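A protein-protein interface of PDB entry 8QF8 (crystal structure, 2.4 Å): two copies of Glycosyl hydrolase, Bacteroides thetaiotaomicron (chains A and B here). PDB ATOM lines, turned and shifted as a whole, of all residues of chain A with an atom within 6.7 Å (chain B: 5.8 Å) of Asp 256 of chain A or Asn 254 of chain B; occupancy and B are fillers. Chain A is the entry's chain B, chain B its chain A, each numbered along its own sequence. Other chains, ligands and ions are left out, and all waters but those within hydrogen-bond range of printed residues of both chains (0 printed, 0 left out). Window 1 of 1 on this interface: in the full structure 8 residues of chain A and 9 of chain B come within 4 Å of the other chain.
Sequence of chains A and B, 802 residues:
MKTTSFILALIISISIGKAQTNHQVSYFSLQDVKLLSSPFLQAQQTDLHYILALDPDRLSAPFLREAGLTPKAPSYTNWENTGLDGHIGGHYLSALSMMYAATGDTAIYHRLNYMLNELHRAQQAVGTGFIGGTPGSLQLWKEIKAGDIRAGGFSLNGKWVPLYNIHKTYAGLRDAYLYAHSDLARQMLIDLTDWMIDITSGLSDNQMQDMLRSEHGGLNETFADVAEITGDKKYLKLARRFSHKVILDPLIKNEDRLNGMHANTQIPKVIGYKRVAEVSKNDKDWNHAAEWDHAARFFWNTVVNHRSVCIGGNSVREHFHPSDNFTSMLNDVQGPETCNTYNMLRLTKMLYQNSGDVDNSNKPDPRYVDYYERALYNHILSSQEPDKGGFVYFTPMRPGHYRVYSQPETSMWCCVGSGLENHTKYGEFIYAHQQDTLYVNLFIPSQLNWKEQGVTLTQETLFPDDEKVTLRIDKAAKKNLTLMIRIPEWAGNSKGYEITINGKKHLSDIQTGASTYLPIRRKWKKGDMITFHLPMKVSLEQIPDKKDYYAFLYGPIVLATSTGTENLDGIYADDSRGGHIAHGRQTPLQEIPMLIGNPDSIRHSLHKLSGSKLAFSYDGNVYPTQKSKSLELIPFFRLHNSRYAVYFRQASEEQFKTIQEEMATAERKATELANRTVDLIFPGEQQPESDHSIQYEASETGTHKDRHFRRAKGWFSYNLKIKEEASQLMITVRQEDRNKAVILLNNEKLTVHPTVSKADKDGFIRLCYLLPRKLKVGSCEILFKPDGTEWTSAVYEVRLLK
Glu 255 of chain A touches Asp 256 of chain B, but with the chains exchanged Asp 256 of chain A does not touch Glu 255 of chain B (5.1 Å).
Asp 256 of chain A touches Asn 254 of chain B, but with the chains exchanged Asn 254 of chain A does not touch Asp 256 of chain B (6.1 Å).
Positions printed for both chains: 250, 251, 254, 255, 256 and 298.
Of the 5 pairs that touch across the chains among the printed residues, none has its exchanged pair printed and touching as well.
Of the 17 printed residues of chain A, 4 touch a printed residue of chain B.
Among the printed residues, pairs that only touch across the chains: Asp 256 of chain A with Asn 254 of chain B and Arg 257 of chain A with Asp 256 of chain B.
OD1 of Asn 254 of chain B sits at hydrogen-bond distance from NE2 of His 294 of chain B (3.0 Å).
The side-chain carboxylate of Asp 256 of chain A is in salt-bridge range of the guanidinium group of Arg 307 of chain A, at 2.7 Å.
N of Glu 255 of chain B lies within hydrogen-bond range of O of Pro 250 of chain B (3.0 Å).
O of Pro 250 of chain A lies within hydrogen-bond range of N of Glu 255 of chain A, at 3.0 Å.
The side-chain carboxylate of Asp 256 of chain A sits at hydrogen-bond distance from the side-chain hydroxyl of Thr 302 of chain A, 2.5 Å away.
The side-chain carboxylate (OD1) of Asp 256 of chain A is in hydrogen-bond range of the backbone NH (N) of Leu 258 of chain A (3.0 Å).
Of the printed residues of chain B, Arg 257 of chain A touches Glu 255 (3.3 Å) and Asp 256 (3.9 Å).
His 306 of chain A touches none of the printed residues of chain B.
Of chain A, only Asp 256 (3.8 Å) comes within 4 Å of Asn 254 of chain B.
Of the printed residues of chain A, His 294 of chain B touches Asp 324.
The nearest printed residue of chain A that does not touch Glu 255 of chain B is Asp 256 of chain A (5.1 Å).
The side-chain carboxylate of Glu 255 of chain A sits close to the backbone carbonyl oxygen of Asp 256 of chain B (3.4 Å).
The guanidinium group (NE) of Arg 257 of chain A is in salt-bridge range of the side-chain carboxylate (OE2) of Glu 255 of chain B, at 3.9 Å.
The side-chain carboxylate (OD2) of Asp 324 of chain A sits close to a ring nitrogen (NE2) of His 294 of chain B (3.5 Å).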
ATOM      1  N   PRO A 250       9.125 -22.904  26.174  1.00  0.00           N
ATOM      2  CA  PRO A 250       9.850 -21.662  25.876  1.00  0.00           C
ATOM      3  C   PRO A 250       9.045 -20.369  26.030  1.00  0.00           C
ATOM      4  O   PRO A 250       9.562 -19.385  26.567  1.00  0.00           O
ATOM      5  CB  PRO A 250      10.295 -21.850  24.415  1.00  0.00           C
ATOM      6  CG  PRO A 250      10.402 -23.347  24.253  1.00  0.00           C
ATOM      7  CD  PRO A 250       9.274 -23.899  25.095  1.00  0.00           C
ATOM      8  N   LEU A 251       7.780 -20.382  25.580  1.00  0.00           N
ATOM      9  CA  LEU A 251       6.926 -19.201  25.616  1.00  0.00           C
ATOM     10  C   LEU A 251       6.600 -18.778  27.054  1.00  0.00           C
ATOM     11  O   LEU A 251       6.435 -17.585  27.304  1.00  0.00           O
ATOM     12  CB  LEU A 251       5.651 -19.477  24.811  1.00  0.00           C
ATOM     13  CG  LEU A 251       5.846 -19.692  23.308  1.00  0.00           C
ATOM     14  CD1 LEU A 251       4.557 -20.178  22.656  1.00  0.00           C
ATOM     15  CD2 LEU A 251       6.324 -18.420  22.619  1.00  0.00           C
ATOM     16  N   ASN A 254       9.464 -16.502  28.164  1.00  0.00           N
ATOM     17  CA  ASN A 254       9.722 -15.348  27.306  1.00  0.00           C
ATOM     18  C   ASN A 254      10.885 -15.622  26.347  1.00  0.00           C
ATOM     19  O   ASN A 254      11.771 -14.785  26.191  1.00  0.00           O
ATOM     20  CB  ASN A 254       9.970 -14.056  28.102  1.00  0.00           C
ATOM     21  CG  ASN A 254       8.846 -13.700  29.051  1.00  0.00           C
ATOM     22  OD1 ASN A 254       7.914 -12.999  28.669  1.00  0.00           O
ATOM     23  ND2 ASN A 254       8.917 -14.184  30.279  1.00  0.00           N
ATOM     24  N   GLU A 255      10.851 -16.788  25.688  1.00  0.00           N
ATOM     25  CA  GLU A 255      11.877 -17.199  24.742  1.00  0.00           C
ATOM     26  C   GLU A 255      11.216 -17.435  23.386  1.00  0.00           C
ATOM     27  O   GLU A 255      10.274 -18.228  23.298  1.00  0.00           O
ATOM     28  CB  GLU A 255      12.576 -18.465  25.242  1.00  0.00           C
ATOM     29  CG  GLU A 255      13.291 -18.294  26.578  1.00  0.00           C
ATOM     30  CD  GLU A 255      13.677 -19.579  27.311  1.00  0.00           C
ATOM     31  OE1 GLU A 255      13.159 -20.668  26.943  1.00  0.00           O
ATOM     32  OE2 GLU A 255      14.513 -19.499  28.250  1.00  0.00           O
ATOM     33  N   ASP A 256      11.690 -16.707  22.357  1.00  0.00           N
ATOM     34  CA  ASP A 256      11.260 -16.881  20.976  1.00  0.00           C
ATOM     35  C   ASP A 256      12.183 -17.887  20.288  1.00  0.00           C
ATOM     36  O   ASP A 256      13.337 -17.570  20.007  1.00  0.00           O
ATOM     37  CB  ASP A 256      11.275 -15.551  20.214  1.00  0.00           C
ATOM     38  CG  ASP A 256      10.656 -15.603  18.821  1.00  0.00           C
ATOM     39  OD1 ASP A 256      10.841 -16.625  18.118  1.00  0.00           O
ATOM     40  OD2 ASP A 256      10.027 -14.600  18.423  1.00  0.00           O
ATOM     41  N   ARG A 257      11.652 -19.079  19.985  1.00  0.00           N
ATOM     42  CA  ARG A 257      12.416 -20.138  19.339  1.00  0.00           C
ATOM     43  C   ARG A 257      11.790 -20.493  17.992  1.00  0.00           C
ATOM     44  O   ARG A 257      12.038 -21.576  17.480  1.00  0.00           O
ATOM     45  CB  ARG A 257      12.461 -21.363  20.259  1.00  0.00           C
ATOM     46  CG  ARG A 257      12.912 -21.052  21.678  1.00  0.00           C
ATOM     47  CD  ARG A 257      14.408 -20.833  21.748  1.00  0.00           C
ATOM     48  NE  ARG A 257      14.889 -20.342  23.036  1.00  0.00           N
ATOM     49  CZ  ARG A 257      15.163 -21.089  24.109  1.00  0.00           C
ATOM     50  NH1 ARG A 257      14.776 -22.356  24.188  1.00  0.00           N
ATOM     51  NH2 ARG A 257      15.810 -20.540  25.129  1.00  0.00           N
ATOM     52  N   LEU A 258      11.053 -19.544  17.396  1.00  0.00           N
ATOM     53  CA  LEU A 258      10.120 -19.832  16.316  1.00  0.00           C
ATOM     54  C   LEU A 258      10.824 -19.920  14.966  1.00  0.00           C
ATOM     55  O   LEU A 258      10.210 -20.405  14.018  1.00  0.00           O
ATOM     56  CB  LEU A 258       9.037 -18.746  16.272  1.00  0.00           C
ATOM     57  CG  LEU A 258       8.204 -18.559  17.541  1.00  0.00           C
ATOM     58  CD1 LEU A 258       7.262 -17.377  17.381  1.00  0.00           C
ATOM     59  CD2 LEU A 258       7.420 -19.818  17.893  1.00  0.00           C
ATOM     60  N   ASN A 259      12.073 -19.436  14.868  1.00  0.00           N
ATOM     61  CA  ASN A 259      12.861 -19.482  13.639  1.00  0.00           C
ATOM     62  C   ASN A 259      12.883 -20.900  13.075  1.00  0.00           C
ATOM     63  O   ASN A 259      13.176 -21.844  13.806  1.00  0.00           O
ATOM     64  CB  ASN A 259      14.288 -18.962  13.874  1.00  0.00           C
ATOM     65  CG  ASN A 259      14.340 -17.456  14.029  1.00  0.00           C
ATOM     66  OD1 ASN A 259      13.340 -16.774  13.822  1.00  0.00           O
ATOM     67  ND2 ASN A 259      15.493 -16.913  14.372  1.00  0.00           N
ATOM     68  N   PHE A 298       3.052 -13.263  25.376  1.00  0.00           N
ATOM     69  CA  PHE A 298       4.416 -13.149  24.881  1.00  0.00           C
ATOM     70  C   PHE A 298       4.502 -13.552  23.408  1.00  0.00           C
ATOM     71  O   PHE A 298       5.158 -12.857  22.636  1.00  0.00           O
ATOM     72  CB  PHE A 298       5.393 -13.999  25.702  1.00  0.00           C
ATOM     73  CG  PHE A 298       6.750 -14.114  25.058  1.00  0.00           C
ATOM     74  CD1 PHE A 298       7.593 -13.010  24.992  1.00  0.00           C
ATOM     75  CD2 PHE A 298       7.146 -15.288  24.427  1.00  0.00           C
ATOM     76  CE1 PHE A 298       8.829 -13.098  24.367  1.00  0.00           C
ATOM     77  CE2 PHE A 298       8.380 -15.373  23.799  1.00  0.00           C
ATOM     78  CZ  PHE A 298       9.218 -14.278  23.765  1.00  0.00           C
ATOM     79  N   PHE A 299       3.878 -14.685  23.041  1.00  0.00           N
ATOM     80  CA  PHE A 299       3.847 -15.159  21.663  1.00  0.00           C
ATOM     81  C   PHE A 299       3.301 -14.079  20.729  1.00  0.00           C
ATOM     82  O   PHE A 299       3.903 -13.802  19.694  1.00  0.00           O
ATOM     83  CB  PHE A 299       2.971 -16.410  21.519  1.00  0.00           C
ATOM     84  CG  PHE A 299       2.883 -16.955  20.115  1.00  0.00           C
ATOM     85  CD1 PHE A 299       3.851 -17.819  19.628  1.00  0.00           C
ATOM     86  CD2 PHE A 299       1.848 -16.577  19.267  1.00  0.00           C
ATOM     87  CE1 PHE A 299       3.764 -18.324  18.336  1.00  0.00           C
ATOM     88  CE2 PHE A 299       1.767 -17.065  17.970  1.00  0.00           C
ATOM     89  CZ  PHE A 299       2.725 -17.940  17.507  1.00  0.00           C
ATOM     90  N   THR A 302       5.865 -11.159  20.300  1.00  0.00           N
ATOM     91  CA  THR A 302       7.054 -11.403  19.490  1.00  0.00           C
ATOM     92  C   THR A 302       6.689 -11.506  18.001  1.00  0.00           C
ATOM     93  O   THR A 302       7.420 -10.998  17.155  1.00  0.00           O
ATOM     94  CB  THR A 302       7.851 -12.601  20.031  1.00  0.00           C
ATOM     95  OG1 THR A 302       9.191 -12.526  19.554  1.00  0.00           O
ATOM     96  CG2 THR A 302       7.292 -13.950  19.641  1.00  0.00           C
ATOM     97  N   VAL A 303       5.563 -12.150  17.669  1.00  0.00           N
ATOM     98  CA  VAL A 303       5.135 -12.296  16.282  1.00  0.00           C
ATOM     99  C   VAL A 303       4.731 -10.938  15.702  1.00  0.00           C
ATOM    100  O   VAL A 303       5.115 -10.624  14.584  1.00  0.00           O
ATOM    101  CB  VAL A 303       4.011 -13.341  16.137  1.00  0.00           C
ATOM    102  CG1 VAL A 303       3.410 -13.364  14.736  1.00  0.00           C
ATOM    103  CG2 VAL A 303       4.505 -14.733  16.515  1.00  0.00           C
ATOM    104  N   HIS A 306       7.990  -8.290  15.932  1.00  0.00           N
ATOM    105  CA  HIS A 306       9.231  -8.692  15.278  1.00  0.00           C
ATOM    106  C   HIS A 306       9.050  -9.463  13.964  1.00  0.00           C
ATOM    107  O   HIS A 306       9.973  -9.438  13.163  1.00  0.00           O
ATOM    108  CB  HIS A 306      10.124  -9.517  16.213  1.00  0.00           C
ATOM    109  CG  HIS A 306      10.481  -8.823  17.477  1.00  0.00           C
ATOM    110  ND1 HIS A 306      11.192  -7.643  17.498  1.00  0.00           N
ATOM    111  CD2 HIS A 306      10.231  -9.133  18.754  1.00  0.00           C
ATOM    112  CE1 HIS A 306      11.365  -7.264  18.758  1.00  0.00           C
ATOM    113  NE2 HIS A 306      10.783  -8.151  19.535  1.00  0.00           N
ATOM    114  N   ARG A 307       7.923 -10.159  13.733  1.00  0.00           N
ATOM    115  CA  ARG A 307       7.831 -11.105  12.620  1.00  0.00           C
ATOM    116  C   ARG A 307       6.737 -10.742  11.619  1.00  0.00           C
ATOM    117  O   ARG A 307       6.473 -11.531  10.715  1.00  0.00           O
ATOM    118  CB  ARG A 307       7.596 -12.524  13.145  1.00  0.00           C
ATOM    119  CG  ARG A 307       8.689 -13.019  14.080  1.00  0.00           C
ATOM    120  CD  ARG A 307       8.368 -14.354  14.702  1.00  0.00           C
ATOM    121  NE  ARG A 307       9.514 -14.904  15.408  1.00  0.00           N
ATOM    122  CZ  ARG A 307      10.600 -15.421  14.843  1.00  0.00           C
ATOM    123  NH1 ARG A 307      10.716 -15.526  13.527  1.00  0.00           N
ATOM    124  NH2 ARG A 307      11.580 -15.846  15.618  1.00  0.00           N
ATOM    125  N   PRO A 322      14.150 -15.826  10.214  1.00  0.00           N
ATOM    126  CA  PRO A 322      14.711 -14.981  11.272  1.00  0.00           C
ATOM    127  C   PRO A 322      14.181 -13.548  11.244  1.00  0.00           C
ATOM    128  O   PRO A 322      13.959 -12.989  10.173  1.00  0.00           O
ATOM    129  CB  PRO A 322      16.227 -15.008  11.019  1.00  0.00           C
ATOM    130  CG  PRO A 322      16.441 -16.306  10.269  1.00  0.00           C
ATOM    131  CD  PRO A 322      15.206 -16.467   9.409  1.00  0.00           C
ATOM    132  N   SER A 323      13.994 -12.971  12.437  1.00  0.00           N
ATOM    133  CA  SER A 323      13.376 -11.664  12.581  1.00  0.00           C
ATOM    134  C   SER A 323      14.376 -10.530  12.323  1.00  0.00           C
ATOM    135  O   SER A 323      13.962  -9.375  12.237  1.00  0.00           O
ATOM    136  CB  SER A 323      12.699 -11.555  13.922  1.00  0.00           C
ATOM    137  OG  SER A 323      13.635 -11.493  14.978  1.00  0.00           O
ATOM    138  N   ASP A 324      15.676 -10.853  12.192  1.00  0.00           N
ATOM    139  CA  ASP A 324      16.695  -9.913  11.742  1.00  0.00           C
ATOM    140  C   ASP A 324      17.013 -10.057  10.247  1.00  0.00           C
ATOM    141  O   ASP A 324      17.980  -9.450   9.798  1.00  0.00           O
ATOM    142  CB  ASP A 324      17.967 -10.044  12.590  1.00  0.00           C
ATOM    143  CG  ASP A 324      18.713 -11.367  12.502  1.00  0.00           C
ATOM    144  OD1 ASP A 324      18.108 -12.372  12.092  1.00  0.00           O
ATOM    145  OD2 ASP A 324      19.907 -11.384  12.863  1.00  0.00           O
ATOM    146  N   PRO B 250      24.031 -20.183  21.306  1.00  0.00           N
ATOM    147  CA  PRO B 250      22.673 -19.714  21.601  1.00  0.00           C
ATOM    148  C   PRO B 250      22.401 -18.245  21.263  1.00  0.00           C
ATOM    149  O   PRO B 250      21.333 -17.932  20.742  1.00  0.00           O
ATOM    150  CB  PRO B 250      22.537 -19.967  23.110  1.00  0.00           C
ATOM    151  CG  PRO B 250      23.425 -21.163  23.339  1.00  0.00           C
ATOM    152  CD  PRO B 250      24.629 -20.861  22.469  1.00  0.00           C
ATOM    153  N   LEU B 251      23.370 -17.359  21.528  1.00  0.00           N
ATOM    154  CA  LEU B 251      23.205 -15.929  21.288  1.00  0.00           C
ATOM    155  C   LEU B 251      23.099 -15.612  19.791  1.00  0.00           C
ATOM    156  O   LEU B 251      22.412 -14.664  19.420  1.00  0.00           O
ATOM    157  CB  LEU B 251      24.371 -15.166  21.933  1.00  0.00           C
ATOM    158  CG  LEU B 251      24.466 -15.249  23.457  1.00  0.00           C
ATOM    159  CD1 LEU B 251      25.780 -14.667  23.952  1.00  0.00           C
ATOM    160  CD2 LEU B 251      23.307 -14.529  24.126  1.00  0.00           C
ATOM    161  N   ILE B 252      23.759 -16.396  18.927  1.00  0.00           N
ATOM    162  CA  ILE B 252      23.606 -16.264  17.479  1.00  0.00           C
ATOM    163  C   ILE B 252      22.147 -16.508  17.062  1.00  0.00           C
ATOM    164  O   ILE B 252      21.664 -15.829  16.157  1.00  0.00           O
ATOM    165  CB  ILE B 252      24.605 -17.181  16.732  1.00  0.00           C
ATOM    166  CG1 ILE B 252      26.040 -16.659  16.876  1.00  0.00           C
ATOM    167  CG2 ILE B 252      24.222 -17.353  15.264  1.00  0.00           C
ATOM    168  CD1 ILE B 252      27.129 -17.602  16.402  1.00  0.00           C
ATOM    169  N   LYS B 253      21.456 -17.446  17.734  1.00  0.00           N
ATOM    170  CA  LYS B 253      20.085 -17.821  17.404  1.00  0.00           C
ATOM    171  C   LYS B 253      19.041 -17.103  18.269  1.00  0.00           C
ATOM    172  O   LYS B 253      17.899 -17.544  18.298  1.00  0.00           O
ATOM    173  CB  LYS B 253      19.926 -19.341  17.552  1.00  0.00           C
ATOM    174  CG  LYS B 253      20.893 -20.184  16.729  1.00  0.00           C
ATOM    175  CD  LYS B 253      20.433 -21.616  16.489  1.00  0.00           C
ATOM    176  CE  LYS B 253      20.370 -22.464  17.743  1.00  0.00           C
ATOM    177  NZ  LYS B 253      20.072 -23.876  17.406  1.00  0.00           N
ATOM    178  N   ASN B 254      19.403 -15.996  18.943  1.00  0.00           N
ATOM    179  CA  ASN B 254      18.474 -15.192  19.736  1.00  0.00           C
ATOM    180  C   ASN B 254      17.846 -16.017  20.866  1.00  0.00           C
ATOM    181  O   ASN B 254      16.638 -15.955  21.083  1.00  0.00           O
ATOM    182  CB  ASN B 254      17.382 -14.527  18.888  1.00  0.00           C
ATOM    183  CG  ASN B 254      17.928 -13.658  17.778  1.00  0.00           C
ATOM    184  OD1 ASN B 254      18.155 -12.469  17.986  1.00  0.00           O
ATOM    185  ND2 ASN B 254      18.152 -14.236  16.608  1.00  0.00           N
ATOM    186  N   GLU B 255      18.686 -16.755  21.601  1.00  0.00           N
ATOM    187  CA  GLU B 255      18.259 -17.594  22.708  1.00  0.00           C
ATOM    188  C   GLU B 255      18.982 -17.133  23.972  1.00  0.00           C
ATOM    189  O   GLU B 255      20.214 -17.084  23.999  1.00  0.00           O
ATOM    190  CB  GLU B 255      18.557 -19.065  22.410  1.00  0.00           C
ATOM    191  CG  GLU B 255      17.825 -19.586  21.181  1.00  0.00           C
ATOM    192  CD  GLU B 255      18.002 -21.057  20.853  1.00  0.00           C
ATOM    193  OE1 GLU B 255      18.963 -21.675  21.370  1.00  0.00           O
ATOM    194  OE2 GLU B 255      17.168 -21.585  20.087  1.00  0.00           O
ATOM    195  N   ASP B 256      18.191 -16.762  24.990  1.00  0.00           N
ATOM    196  CA  ASP B 256      18.679 -16.427  26.317  1.00  0.00           C
ATOM    197  C   ASP B 256      18.616 -17.676  27.195  1.00  0.00           C
ATOM    198  O   ASP B 256      17.532 -18.073  27.622  1.00  0.00           O
ATOM    199  CB  ASP B 256      17.846 -15.295  26.925  1.00  0.00           C
ATOM    200  CG  ASP B 256      18.386 -14.745  28.234  1.00  0.00           C
ATOM    201  OD1 ASP B 256      18.960 -15.537  29.026  1.00  0.00           O
ATOM    202  OD2 ASP B 256      18.186 -13.533  28.483  1.00  0.00           O
ATOM    203  N   HIS B 294      25.786  -9.617  15.731  1.00  0.00           N
ATOM    204  CA  HIS B 294      24.389  -9.816  16.089  1.00  0.00           C
ATOM    205  C   HIS B 294      24.240 -10.500  17.454  1.00  0.00           C
ATOM    206  O   HIS B 294      23.383 -10.099  18.235  1.00  0.00           O
ATOM    207  CB  HIS B 294      23.624 -10.595  15.010  1.00  0.00           C
ATOM    208  CG  HIS B 294      22.271 -11.020  15.491  1.00  0.00           C
ATOM    209  ND1 HIS B 294      21.278 -10.127  15.845  1.00  0.00           N
ATOM    210  CD2 HIS B 294      21.791 -12.248  15.767  1.00  0.00           C
ATOM    211  CE1 HIS B 294      20.219 -10.802  16.266  1.00  0.00           C
ATOM    212  NE2 HIS B 294      20.508 -12.093  16.228  1.00  0.00           N
ATOM    213  N   PHE B 298      22.130  -8.965  20.609  1.00  0.00           N
ATOM    214  CA  PHE B 298      21.066  -9.716  21.256  1.00  0.00           C
ATOM    215  C   PHE B 298      21.336  -9.857  22.752  1.00  0.00           C
ATOM    216  O   PHE B 298      20.424  -9.665  23.547  1.00  0.00           O
ATOM    217  CB  PHE B 298      20.885 -11.108  20.636  1.00  0.00           C
ATOM    218  CG  PHE B 298      19.978 -11.996  21.449  1.00  0.00           C
ATOM    219  CD1 PHE B 298      18.618 -11.724  21.544  1.00  0.00           C
ATOM    220  CD2 PHE B 298      20.500 -13.027  22.217  1.00  0.00           C
ATOM    221  CE1 PHE B 298      17.790 -12.510  22.333  1.00  0.00           C
ATOM    222  CE2 PHE B 298      19.673 -13.808  23.012  1.00  0.00           C
ATOM    223  CZ  PHE B 298      18.318 -13.545  23.074  1.00  0.00           C
